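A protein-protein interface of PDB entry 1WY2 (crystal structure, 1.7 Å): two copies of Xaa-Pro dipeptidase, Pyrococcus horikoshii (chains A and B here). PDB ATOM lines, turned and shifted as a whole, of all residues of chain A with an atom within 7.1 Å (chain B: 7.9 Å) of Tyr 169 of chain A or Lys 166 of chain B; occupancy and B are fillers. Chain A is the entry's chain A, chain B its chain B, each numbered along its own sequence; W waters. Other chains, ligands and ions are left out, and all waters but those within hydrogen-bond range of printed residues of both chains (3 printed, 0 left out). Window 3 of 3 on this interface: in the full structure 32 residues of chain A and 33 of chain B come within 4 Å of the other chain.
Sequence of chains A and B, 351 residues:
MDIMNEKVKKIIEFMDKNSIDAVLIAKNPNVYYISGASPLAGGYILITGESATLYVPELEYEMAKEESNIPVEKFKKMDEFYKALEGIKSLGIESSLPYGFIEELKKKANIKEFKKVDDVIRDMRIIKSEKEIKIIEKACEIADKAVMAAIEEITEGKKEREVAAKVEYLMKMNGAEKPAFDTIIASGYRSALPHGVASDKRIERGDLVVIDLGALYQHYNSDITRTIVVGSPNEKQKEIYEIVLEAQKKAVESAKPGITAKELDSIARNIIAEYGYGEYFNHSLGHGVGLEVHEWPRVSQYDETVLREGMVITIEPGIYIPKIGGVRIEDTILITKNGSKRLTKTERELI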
ATOM      1  N   VAL A 163      10.253 -12.484  36.996  1.00  0.00           N
ATOM      2  CA  VAL A 163       9.134 -12.385  36.069  1.00  0.00           C
ATOM      3  C   VAL A 163       9.470 -11.250  35.103  1.00  0.00           C
ATOM      4  O   VAL A 163       9.298 -11.373  33.888  1.00  0.00           O
ATOM      5  CB  VAL A 163       7.811 -12.057  36.807  1.00  0.00           C
ATOM      6  CG1 VAL A 163       6.698 -11.791  35.796  1.00  0.00           C
ATOM      7  CG2 VAL A 163       7.431 -13.217  37.721  1.00  0.00           C
ATOM      8  N   ALA A 164       9.960 -10.144  35.653  1.00  0.00           N
ATOM      9  CA  ALA A 164      10.327  -8.993  34.838  1.00  0.00           C
ATOM     10  C   ALA A 164      11.390  -9.385  33.819  1.00  0.00           C
ATOM     11  O   ALA A 164      11.298  -9.033  32.644  1.00  0.00           O
ATOM     12  CB  ALA A 164      10.839  -7.861  35.727  1.00  0.00           C
ATOM     13  N   ALA A 165      12.396 -10.127  34.269  1.00  0.00           N
ATOM     14  CA  ALA A 165      13.469 -10.548  33.380  1.00  0.00           C
ATOM     15  C   ALA A 165      12.934 -11.369  32.208  1.00  0.00           C
ATOM     16  O   ALA A 165      13.340 -11.170  31.064  1.00  0.00           O
ATOM     17  CB  ALA A 165      14.502 -11.358  34.160  1.00  0.00           C
ATOM     18  N   LYS A 166      12.007 -12.278  32.494  1.00  0.00           N
ATOM     19  CA  LYS A 166      11.436 -13.135  31.463  1.00  0.00           C
ATOM     20  C   LYS A 166      10.646 -12.370  30.403  1.00  0.00           C
ATOM     21  O   LYS A 166      10.801 -12.627  29.209  1.00  0.00           O
ATOM     22  CB  LYS A 166      10.536 -14.196  32.106  1.00  0.00           C
ATOM     23  CG  LYS A 166       9.943 -15.211  31.134  1.00  0.00           C
ATOM     24  CD  LYS A 166      11.001 -16.157  30.586  1.00  0.00           C
ATOM     25  CE  LYS A 166      10.382 -17.222  29.691  1.00  0.00           C
ATOM     26  NZ  LYS A 166       9.379 -18.052  30.423  1.00  0.00           N
ATOM     27  N   VAL A 167       9.805 -11.429  30.826  1.00  0.00           N
ATOM     28  CA  VAL A 167       9.004 -10.687  29.859  1.00  0.00           C
ATOM     29  C   VAL A 167       9.808  -9.642  29.101  1.00  0.00           C
ATOM     30  O   VAL A 167       9.463  -9.289  27.978  1.00  0.00           O
ATOM     31  CB  VAL A 167       7.769 -10.022  30.523  1.00  0.00           C
ATOM     32  CG1 VAL A 167       6.948 -11.077  31.245  1.00  0.00           C
ATOM     33  CG2 VAL A 167       8.198  -8.924  31.468  1.00  0.00           C
ATOM     34  N   GLU A 168      10.883  -9.146  29.703  1.00  0.00           N
ATOM     35  CA  GLU A 168      11.705  -8.166  29.009  1.00  0.00           C
ATOM     36  C   GLU A 168      12.484  -8.889  27.918  1.00  0.00           C
ATOM     37  O   GLU A 168      12.753  -8.327  26.857  1.00  0.00           O
ATOM     38  CB  GLU A 168      12.634  -7.453  29.992  1.00  0.00           C
ATOM     39  CG  GLU A 168      11.851  -6.552  30.958  1.00  0.00           C
ATOM     40  CD  GLU A 168      12.723  -5.827  31.959  1.00  0.00           C
ATOM     41  OE1 GLU A 168      13.849  -6.300  32.223  1.00  0.00           O
ATOM     42  OE2 GLU A 168      12.268  -4.791  32.500  1.00  0.00           O
ATOM     43  N   TYR A 169      12.836 -10.145  28.178  1.00  0.00           N
ATOM     44  CA  TYR A 169      13.540 -10.952  27.190  1.00  0.00           C
ATOM     45  C   TYR A 169      12.571 -11.220  26.042  1.00  0.00           C
ATOM     46  O   TYR A 169      12.937 -11.126  24.875  1.00  0.00           O
ATOM     47  CB  TYR A 169      14.008 -12.274  27.810  1.00  0.00           C
ATOM     48  CG  TYR A 169      14.579 -13.263  26.814  1.00  0.00           C
ATOM     49  CD1 TYR A 169      13.768 -14.232  26.222  1.00  0.00           C
ATOM     50  CD2 TYR A 169      15.926 -13.224  26.457  1.00  0.00           C
ATOM     51  CE1 TYR A 169      14.287 -15.142  25.296  1.00  0.00           C
ATOM     52  CE2 TYR A 169      16.453 -14.126  25.532  1.00  0.00           C
ATOM     53  CZ  TYR A 169      15.627 -15.082  24.957  1.00  0.00           C
ATOM     54  OH  TYR A 169      16.149 -15.975  24.046  1.00  0.00           O
ATOM     55  N   LEU A 170      11.325 -11.544  26.380  1.00  0.00           N
ATOM     56  CA  LEU A 170      10.316 -11.813  25.363  1.00  0.00           C
ATOM     57  C   LEU A 170      10.098 -10.598  24.465  1.00  0.00           C
ATOM     58  O   LEU A 170       9.989 -10.733  23.244  1.00  0.00           O
ATOM     59  CB  LEU A 170       8.987 -12.215  26.017  1.00  0.00           C
ATOM     60  CG  LEU A 170       7.821 -12.452  25.052  1.00  0.00           C
ATOM     61  CD1 LEU A 170       8.099 -13.691  24.208  1.00  0.00           C
ATOM     62  CD2 LEU A 170       6.525 -12.621  25.832  1.00  0.00           C
ATOM     63  N   MET A 171      10.040  -9.410  25.061  1.00  0.00           N
ATOM     64  CA  MET A 171       9.830  -8.199  24.274  1.00  0.00           C
ATOM     65  C   MET A 171      10.963  -7.996  23.271  1.00  0.00           C
ATOM     66  O   MET A 171      10.723  -7.667  22.111  1.00  0.00           O
ATOM     67  CB  MET A 171       9.710  -6.972  25.184  1.00  0.00           C
ATOM     68  CG  MET A 171       8.399  -6.909  25.965  1.00  0.00           C
ATOM     69  SD  MET A 171       8.013  -5.250  26.607  1.00  0.00           S
ATOM     70  CE  MET A 171       9.010  -5.227  28.109  1.00  0.00           C
ATOM     71  N   LYS A 172      12.194  -8.203  23.720  1.00  0.00           N
ATOM     72  CA  LYS A 172      13.354  -8.038  22.849  1.00  0.00           C
ATOM     73  C   LYS A 172      13.346  -9.053  21.714  1.00  0.00           C
ATOM     74  O   LYS A 172      13.675  -8.725  20.571  1.00  0.00           O
ATOM     75  CB  LYS A 172      14.643  -8.191  23.657  1.00  0.00           C
ATOM     76  CG  LYS A 172      14.840  -7.108  24.691  1.00  0.00           C
ATOM     77  CD  LYS A 172      15.955  -7.465  25.660  1.00  0.00           C
ATOM     78  CE  LYS A 172      15.933  -6.543  26.867  1.00  0.00           C
ATOM     79  NZ  LYS A 172      16.964  -6.913  27.876  1.00  0.00           N
ATOM     80  N   MET A 173      12.966 -10.285  22.022  1.00  0.00           N
ATOM     81  CA  MET A 173      12.945 -11.318  21.000  1.00  0.00           C
ATOM     82  C   MET A 173      11.785 -11.123  20.033  1.00  0.00           C
ATOM     83  O   MET A 173      11.719 -11.777  18.992  1.00  0.00           O
ATOM     84  CB  MET A 173      12.899 -12.702  21.653  1.00  0.00           C
ATOM     85  CG  MET A 173      14.152 -13.013  22.473  1.00  0.00           C
ATOM     86  SD  MET A 173      15.695 -13.069  21.505  1.00  0.00           S
ATOM     87  CE  MET A 173      16.103 -11.355  21.333  1.00  0.00           C
ATOM     88  N   ASN A 174      10.880 -10.211  20.377  1.00  0.00           N
ATOM     89  CA  ASN A 174       9.745  -9.910  19.518  1.00  0.00           C
ATOM     90  C   ASN A 174       9.955  -8.618  18.736  1.00  0.00           C
ATOM     91  O   ASN A 174       9.025  -8.097  18.119  1.00  0.00           O
ATOM     92  CB  ASN A 174       8.456  -9.832  20.334  1.00  0.00           C
ATOM     93  CG  ASN A 174       7.832 -11.193  20.552  1.00  0.00           C
ATOM     94  OD1 ASN A 174       7.350 -11.827  19.611  1.00  0.00           O
ATOM     95  ND2 ASN A 174       7.845 -11.657  21.792  1.00  0.00           N
ATOM     96  N   GLY A 175      11.181  -8.101  18.770  1.00  0.00           N
ATOM     97  CA  GLY A 175      11.490  -6.897  18.017  1.00  0.00           C
ATOM     98  C   GLY A 175      11.751  -5.610  18.775  1.00  0.00           C
ATOM     99  O   GLY A 175      12.255  -4.646  18.195  1.00  0.00           O
ATOM    100  N   PRO A 179      12.978  -2.449  26.987  1.00  0.00           N
ATOM    101  CA  PRO A 179      11.740  -2.033  27.658  1.00  0.00           C
ATOM    102  C   PRO A 179      11.616  -0.512  27.587  1.00  0.00           C
ATOM    103  O   PRO A 179      12.624   0.192  27.590  1.00  0.00           O
ATOM    104  CB  PRO A 179      11.937  -2.526  29.093  1.00  0.00           C
ATOM    105  CG  PRO A 179      12.879  -3.688  28.939  1.00  0.00           C
ATOM    106  CD  PRO A 179      13.862  -3.169  27.921  1.00  0.00           C
ATOM    107  N   ALA B 146      28.100 -12.365  32.961  1.00  0.00           N
ATOM    108  CA  ALA B 146      27.423 -12.055  31.707  1.00  0.00           C
ATOM    109  C   ALA B 146      28.369 -12.171  30.518  1.00  0.00           C
ATOM    110  O   ALA B 146      27.963 -12.613  29.444  1.00  0.00           O
ATOM    111  CB  ALA B 146      26.814 -10.651  31.762  1.00  0.00           C
ATOM    112  N   ALA B 149      28.858 -15.796  29.719  1.00  0.00           N
ATOM    113  CA  ALA B 149      27.637 -16.312  29.110  1.00  0.00           C
ATOM    114  C   ALA B 149      27.562 -15.870  27.648  1.00  0.00           C
ATOM    115  O   ALA B 149      27.118 -16.627  26.779  1.00  0.00           O
ATOM    116  CB  ALA B 149      26.415 -15.809  29.875  1.00  0.00           C
ATOM    117  N   ALA B 150      27.996 -14.641  27.381  1.00  0.00           N
ATOM    118  CA  ALA B 150      27.991 -14.103  26.024  1.00  0.00           C
ATOM    119  C   ALA B 150      28.896 -14.939  25.128  1.00  0.00           C
ATOM    120  O   ALA B 150      28.538 -15.272  24.003  1.00  0.00           O
ATOM    121  CB  ALA B 150      28.471 -12.653  26.028  1.00  0.00           C
ATOM    122  N   GLU B 153      27.223 -18.154  24.293  1.00  0.00           N
ATOM    123  CA  GLU B 153      26.122 -17.937  23.354  1.00  0.00           C
ATOM    124  C   GLU B 153      26.570 -17.634  21.921  1.00  0.00           C
ATOM    125  O   GLU B 153      25.870 -17.958  20.962  1.00  0.00           O
ATOM    126  CB  GLU B 153      25.236 -16.786  23.842  1.00  0.00           C
ATOM    127  CG  GLU B 153      24.423 -17.079  25.096  1.00  0.00           C
ATOM    128  CD  GLU B 153      23.381 -18.165  24.886  1.00  0.00           C
ATOM    129  OE1 GLU B 153      22.877 -18.305  23.753  1.00  0.00           O
ATOM    130  OE2 GLU B 153      23.053 -18.868  25.864  1.00  0.00           O
ATOM    131  N   LYS B 158      24.201 -16.613  14.622  1.00  0.00           N
ATOM    132  CA  LYS B 158      23.349 -15.994  15.631  1.00  0.00           C
ATOM    133  C   LYS B 158      23.384 -14.468  15.564  1.00  0.00           C
ATOM    134  O   LYS B 158      24.431 -13.864  15.331  1.00  0.00           O
ATOM    135  CB  LYS B 158      23.764 -16.463  17.030  1.00  0.00           C
ATOM    136  CG  LYS B 158      22.844 -15.978  18.147  1.00  0.00           C
ATOM    137  CD  LYS B 158      23.171 -16.636  19.481  1.00  0.00           C
ATOM    138  CE  LYS B 158      22.800 -18.116  19.481  1.00  0.00           C
ATOM    139  NZ  LYS B 158      23.098 -18.752  20.792  1.00  0.00           N
ATOM    140  N   GLU B 160      23.506 -10.703  16.830  1.00  0.00           N
ATOM    141  CA  GLU B 160      24.168 -10.057  17.962  1.00  0.00           C
ATOM    142  C   GLU B 160      23.137  -9.730  19.042  1.00  0.00           C
ATOM    143  O   GLU B 160      23.401  -9.876  20.233  1.00  0.00           O
ATOM    144  CB  GLU B 160      24.845  -8.757  17.519  1.00  0.00           C
ATOM    145  CG  GLU B 160      25.824  -8.905  16.367  1.00  0.00           C
ATOM    146  CD  GLU B 160      26.266  -7.563  15.803  1.00  0.00           C
ATOM    147  OE1 GLU B 160      25.484  -6.596  15.903  1.00  0.00           O
ATOM    148  OE2 GLU B 160      27.380  -7.478  15.243  1.00  0.00           O
ATOM    149  N   ARG B 161      21.965  -9.271  18.610  1.00  0.00           N
ATOM    150  CA  ARG B 161      20.887  -8.911  19.527  1.00  0.00           C
ATOM    151  C   ARG B 161      20.371 -10.073  20.364  1.00  0.00           C
ATOM    152  O   ARG B 161      19.880  -9.861  21.473  1.00  0.00           O
ATOM    153  CB  ARG B 161      19.710  -8.307  18.753  1.00  0.00           C
ATOM    154  CG  ARG B 161      19.845  -6.836  18.432  1.00  0.00           C
ATOM    155  CD  ARG B 161      18.712  -6.389  17.510  1.00  0.00           C
ATOM    156  NE  ARG B 161      17.395  -6.776  18.019  1.00  0.00           N
ATOM    157  CZ  ARG B 161      16.809  -6.237  19.085  1.00  0.00           C
ATOM    158  NH1 ARG B 161      17.416  -5.275  19.768  1.00  0.00           N
ATOM    159  NH2 ARG B 161      15.611  -6.659  19.469  1.00  0.00           N
ATOM    160  N   GLU B 162      20.451 -11.292  19.833  1.00  0.00           N
ATOM    161  CA  GLU B 162      19.976 -12.449  20.586  1.00  0.00           C
ATOM    162  C   GLU B 162      20.948 -12.724  21.720  1.00  0.00           C
ATOM    163  O   GLU B 162      20.541 -13.100  22.818  1.00  0.00           O
ATOM    164  CB  GLU B 162      19.864 -13.702  19.710  1.00  0.00           C
ATOM    165  CG  GLU B 162      19.270 -14.881  20.489  1.00  0.00           C
ATOM    166  CD  GLU B 162      19.173 -16.169  19.691  1.00  0.00           C
ATOM    167  OE1 GLU B 162      18.807 -16.114  18.499  1.00  0.00           O
ATOM    168  OE2 GLU B 162      19.446 -17.242  20.271  1.00  0.00           O
ATOM    169  N   VAL B 163      22.235 -12.549  21.440  1.00  0.00           N
ATOM    170  CA  VAL B 163      23.253 -12.758  22.460  1.00  0.00           C
ATOM    171  C   VAL B 163      23.028 -11.719  23.555  1.00  0.00           C
ATOM    172  O   VAL B 163      23.031 -12.044  24.742  1.00  0.00           O
ATOM    173  CB  VAL B 163      24.677 -12.593  21.882  1.00  0.00           C
ATOM    174  CG1 VAL B 163      25.707 -12.681  22.999  1.00  0.00           C
ATOM    175  CG2 VAL B 163      24.943 -13.674  20.837  1.00  0.00           C
ATOM    176  N   ALA B 164      22.824 -10.468  23.150  1.00  0.00           N
ATOM    177  CA  ALA B 164      22.589  -9.388  24.107  1.00  0.00           C
ATOM    178  C   ALA B 164      21.368  -9.660  24.981  1.00  0.00           C
ATOM    179  O   ALA B 164      21.430  -9.518  26.203  1.00  0.00           O
ATOM    180  CB  ALA B 164      22.420  -8.056  23.373  1.00  0.00           C
ATOM    181  N   ALA B 165      20.257 -10.052  24.365  1.00  0.00           N
ATOM    182  CA  ALA B 165      19.050 -10.331  25.138  1.00  0.00           C
ATOM    183  C   ALA B 165      19.292 -11.443  26.152  1.00  0.00           C
ATOM    184  O   ALA B 165      18.861 -11.351  27.300  1.00  0.00           O
ATOM    185  CB  ALA B 165      17.900 -10.712  24.210  1.00  0.00           C
ATOM    186  N   LYS B 166      19.993 -12.489  25.730  1.00  0.00           N
ATOM    187  CA  LYS B 166      20.271 -13.614  26.610  1.00  0.00           C
ATOM    188  C   LYS B 166      21.105 -13.221  27.825  1.00  0.00           C
ATOM    189  O   LYS B 166      20.801 -13.627  28.952  1.00  0.00           O
ATOM    190  CB  LYS B 166      20.988 -14.724  25.837  1.00  0.00           C
ATOM    191  CG  LYS B 166      21.068 -16.045  26.586  1.00  0.00           C
ATOM    192  CD  LYS B 166      19.721 -16.762  26.602  1.00  0.00           C
ATOM    193  CE  LYS B 166      19.355 -17.281  25.215  1.00  0.00           C
ATOM    194  NZ  LYS B 166      18.237 -18.269  25.255  1.00  0.00           N
ATOM    195  N   VAL B 167      22.153 -12.428  27.614  1.00  0.00           N
ATOM    196  CA  VAL B 167      22.988 -12.039  28.743  1.00  0.00           C
ATOM    197  C   VAL B 167      22.345 -10.980  29.634  1.00  0.00           C
ATOM    198  O   VAL B 167      22.635 -10.920  30.826  1.00  0.00           O
ATOM    199  CB  VAL B 167      24.397 -11.579  28.286  1.00  0.00           C
ATOM    200  CG1 VAL B 167      25.082 -12.719  27.534  1.00  0.00           C
ATOM    201  CG2 VAL B 167      24.303 -10.345  27.420  1.00  0.00           C
ATOM    202  N   GLU B 168      21.468 -10.151  29.074  1.00  0.00           N
ATOM    203  CA  GLU B 168      20.800  -9.146  29.894  1.00  0.00           C
ATOM    204  C   GLU B 168      19.817  -9.871  30.804  1.00  0.00           C
ATOM    205  O   GLU B 168      19.596  -9.470  31.946  1.00  0.00           O
ATOM    206  CB  GLU B 168      20.095  -8.117  29.010  1.00  0.00           C
ATOM    207  CG  GLU B 168      21.093  -7.336  28.160  1.00  0.00           C
ATOM    208  CD  GLU B 168      20.449  -6.299  27.265  1.00  0.00           C
ATOM    209  OE1 GLU B 168      19.296  -6.511  26.841  1.00  0.00           O
ATOM    210  OE2 GLU B 168      21.112  -5.282  26.965  1.00  0.00           O
ATOM    211  N   TYR B 169      19.239 -10.950  30.290  1.00  0.00           N
ATOM    212  CA  TYR B 169      18.318 -11.772  31.065  1.00  0.00           C
ATOM    213  C   TYR B 169      19.094 -12.374  32.238  1.00  0.00           C
ATOM    214  O   TYR B 169      18.652 -12.321  33.389  1.00  0.00           O
ATOM    215  CB  TYR B 169      17.751 -12.886  30.182  1.00  0.00           C
ATOM    216  CG  TYR B 169      17.002 -13.965  30.931  1.00  0.00           C
ATOM    217  CD1 TYR B 169      17.607 -15.190  31.221  1.00  0.00           C
ATOM    218  CD2 TYR B 169      15.689 -13.762  31.351  1.00  0.00           C
ATOM    219  CE1 TYR B 169      16.915 -16.187  31.912  1.00  0.00           C
ATOM    220  CE2 TYR B 169      14.989 -14.750  32.038  1.00  0.00           C
ATOM    221  CZ  TYR B 169      15.608 -15.957  32.316  1.00  0.00           C
ATOM    222  OH  TYR B 169      14.913 -16.927  32.996  1.00  0.00           O
ATOM    223  N   LEU B 170      20.262 -12.937  31.939  1.00  0.00           N
ATOM    224  CA  LEU B 170      21.093 -13.551  32.969  1.00  0.00           C
ATOM    225  C   LEU B 170      21.475 -12.553  34.059  1.00  0.00           C
ATOM    226  O   LEU B 170      21.456 -12.884  35.244  1.00  0.00           O
ATOM    227  CB  LEU B 170      22.352 -14.157  32.338  1.00  0.00           C
ATOM    228  CG  LEU B 170      23.365 -14.835  33.268  1.00  0.00           C
ATOM    229  CD1 LEU B 170      24.215 -15.811  32.471  1.00  0.00           C
ATOM    230  CD2 LEU B 170      24.239 -13.791  33.949  1.00  0.00           C
ATOM    231  N   MET B 171      21.812 -11.327  33.671  1.00  0.00           N
ATOM    232  CA  MET B 171      22.185 -10.330  34.665  1.00  0.00           C
ATOM    233  C   MET B 171      21.035 -10.030  35.619  1.00  0.00           C
ATOM    234  O   MET B 171      21.242  -9.932  36.824  1.00  0.00           O
ATOM    235  CB  MET B 171      22.657  -9.035  33.998  1.00  0.00           C
ATOM    236  CG  MET B 171      24.005  -9.163  33.287  1.00  0.00           C
ATOM    237  SD  MET B 171      24.760  -7.551  32.967  1.00  0.00           S
ATOM    238  CE  MET B 171      23.809  -7.020  31.518  1.00  0.00           C
ATOM    239  N   LYS B 172      19.825  -9.900  35.082  1.00  0.00           N
ATOM    240  CA  LYS B 172      18.658  -9.606  35.907  1.00  0.00           C
ATOM    241  C   LYS B 172      18.320 -10.796  36.806  1.00  0.00           C
ATOM    242  O   LYS B 172      17.880 -10.622  37.942  1.00  0.00           O
ATOM    243  CB  LYS B 172      17.465  -9.243  35.015  1.00  0.00           C
ATOM    244  CG  LYS B 172      16.336  -8.538  35.748  1.00  0.00           C
ATOM    245  CD  LYS B 172      15.677  -7.492  34.852  1.00  0.00           C
ATOM    246  CE  LYS B 172      14.676  -6.652  35.618  1.00  0.00           C
ATOM    247  NZ  LYS B 172      14.186  -5.502  34.805  1.00  0.00           N
ATOM    248  N   MET B 173      18.529 -12.007  36.299  1.00  0.00           N
ATOM    249  CA  MET B 173      18.262 -13.201  37.091  1.00  0.00           C
ATOM    250  C   MET B 173      19.279 -13.286  38.230  1.00  0.00           C
ATOM    251  O   MET B 173      19.070 -14.001  39.213  1.00  0.00           O
ATOM    252  CB  MET B 173      18.344 -14.455  36.217  1.00  0.00           C
ATOM    253  CG  MET B 173      17.218 -14.585  35.193  1.00  0.00           C
ATOM    254  SD  MET B 173      15.574 -14.706  35.940  1.00  0.00           S
ATOM    255  CE  MET B 173      15.538 -16.424  36.408  1.00  0.00           C
HETATM  256  O   HOH W   1      17.714  -3.664  27.398  1.00  0.00           O
HETATM  257  O   HOH W   2      13.721  -2.684  33.517  1.00  0.00           O
HETATM  258  O   HOH W   3      16.642  -9.794  27.951  1.00  0.00           O
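OE1 of Glu 168 of chain B lies within salt-bridge range of NZ of Lys 172 of chain A (2.6 Å).
The side-chain amino group of Lys 172 of chain B lies within salt-bridge range of the side-chain carboxylate of Glu 168 of chain A (2.7 Å).
The side-chain hydroxyl (OH) of Tyr 169 of chain A is in hydrogen-bond range of the side-chain amino group (NZ) of Lys 166 of chain B (3.3 Å).
O of Lys 172 of chain A is in hydrogen-bond range of NH2 of Arg 161 of chain B, at 3.0 Å.
The side-chain hydroxyl of Tyr 169 of chain B sits close to the side-chain sulfur of Met 173 of chain B (3.7 Å).
Among the printed residues, pairs that only touch across the chains: Met 173 of chain A with Ala 165 of chain B (3.5 Å), Ala 165 of chain A with Tyr 169 of chain B (3.5 Å), Tyr 169 of chain A with Ala 165 of chain B (3.6 Å), Ala 165 of chain A with Lys 172 of chain B (3.7 Å), Lys 166 of chain A with Tyr 169 of chain B (3.9 Å) and Ala 165 of chain A with Met 173 of chain B (3.9 Å).
Of the printed residues of chain B, Glu 168 of chain A touches Lys 172.
Tyr 169 of chain A touches two residues of chain B.
Glu 160 of chain B touches none of the printed residues of chain A.
Printed residues of chain A within 4 Å of Ala 165 of chain B: Tyr 169 (3.6 Å) and Met 173 (3.5 Å).
Of chain A, only Tyr 169 comes within 4 Å of Lys 166 of chain B.
Of the printed residues of chain A, Tyr 169 of chain B touches Ala 165 and Lys 166.
Leu 170 of chain B touches none of the printed residues of chain A.
Printed residues of chain A within 4 Å of Met 173 of chain B: Ala 165 (3.9 Å).
The nearest residue of chain A that does not touch Lys 166 of chain B is Met 173 of chain A (6.0 Å).
Printed residues of chain A that touch a printed residue of chain B: Ala 165, Lys 166, Glu 168, Tyr 169, Lys 172 and Met 173.
Hydrophobic or aromatic side chains of chain A that line the printed part of chain B: Ala 165, Tyr 169 and Met 173.
Ala 165 of chain A touches Tyr 169 of chain B, and with the chains exchanged Tyr 169 of chain A touches Ala 165 of chain B.
Ala 165 of chain A touches Lys 172 of chain B, but with the chains exchanged Lys 172 of chain A does not touch Ala 165 of chain B (4.1 Å).
Ala 165 of chain A touches Met 173 of chain B, and with the chains exchanged Met 173 of chain A touches Ala 165 of chain B.
Lys 166 of chain A touches Tyr 169 of chain B, and with the chains exchanged Tyr 169 of chain A touches Lys 166 of chain B.
Positions printed for both chains: 163, 164, 165, 166, 167, 168, 169, 170, 171, 172 and 173.
Of the 10 pairs that touch across the chains among the printed residues, 8 have their exchanged pair printed and touching as well.
Water W2 lies within hydrogen-bond range of the side-chain carboxylate of Glu 168 of chain A (2.8 Å) and the side-chain amino group of Lys 172 of chain B (3.1 Å).
Water W3 lies within hydrogen-bond range of the backbone carbonyl oxygen of Ala 165 of chain B (2.8 Å) and the side-chain amino group of Lys 172 of chain A (2.9 Å).
Water W1 bridges the side-chain carboxylate (OE1) of Glu 168 of chain B and the side-chain amino group (NZ) of Lys 172 of chain A.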
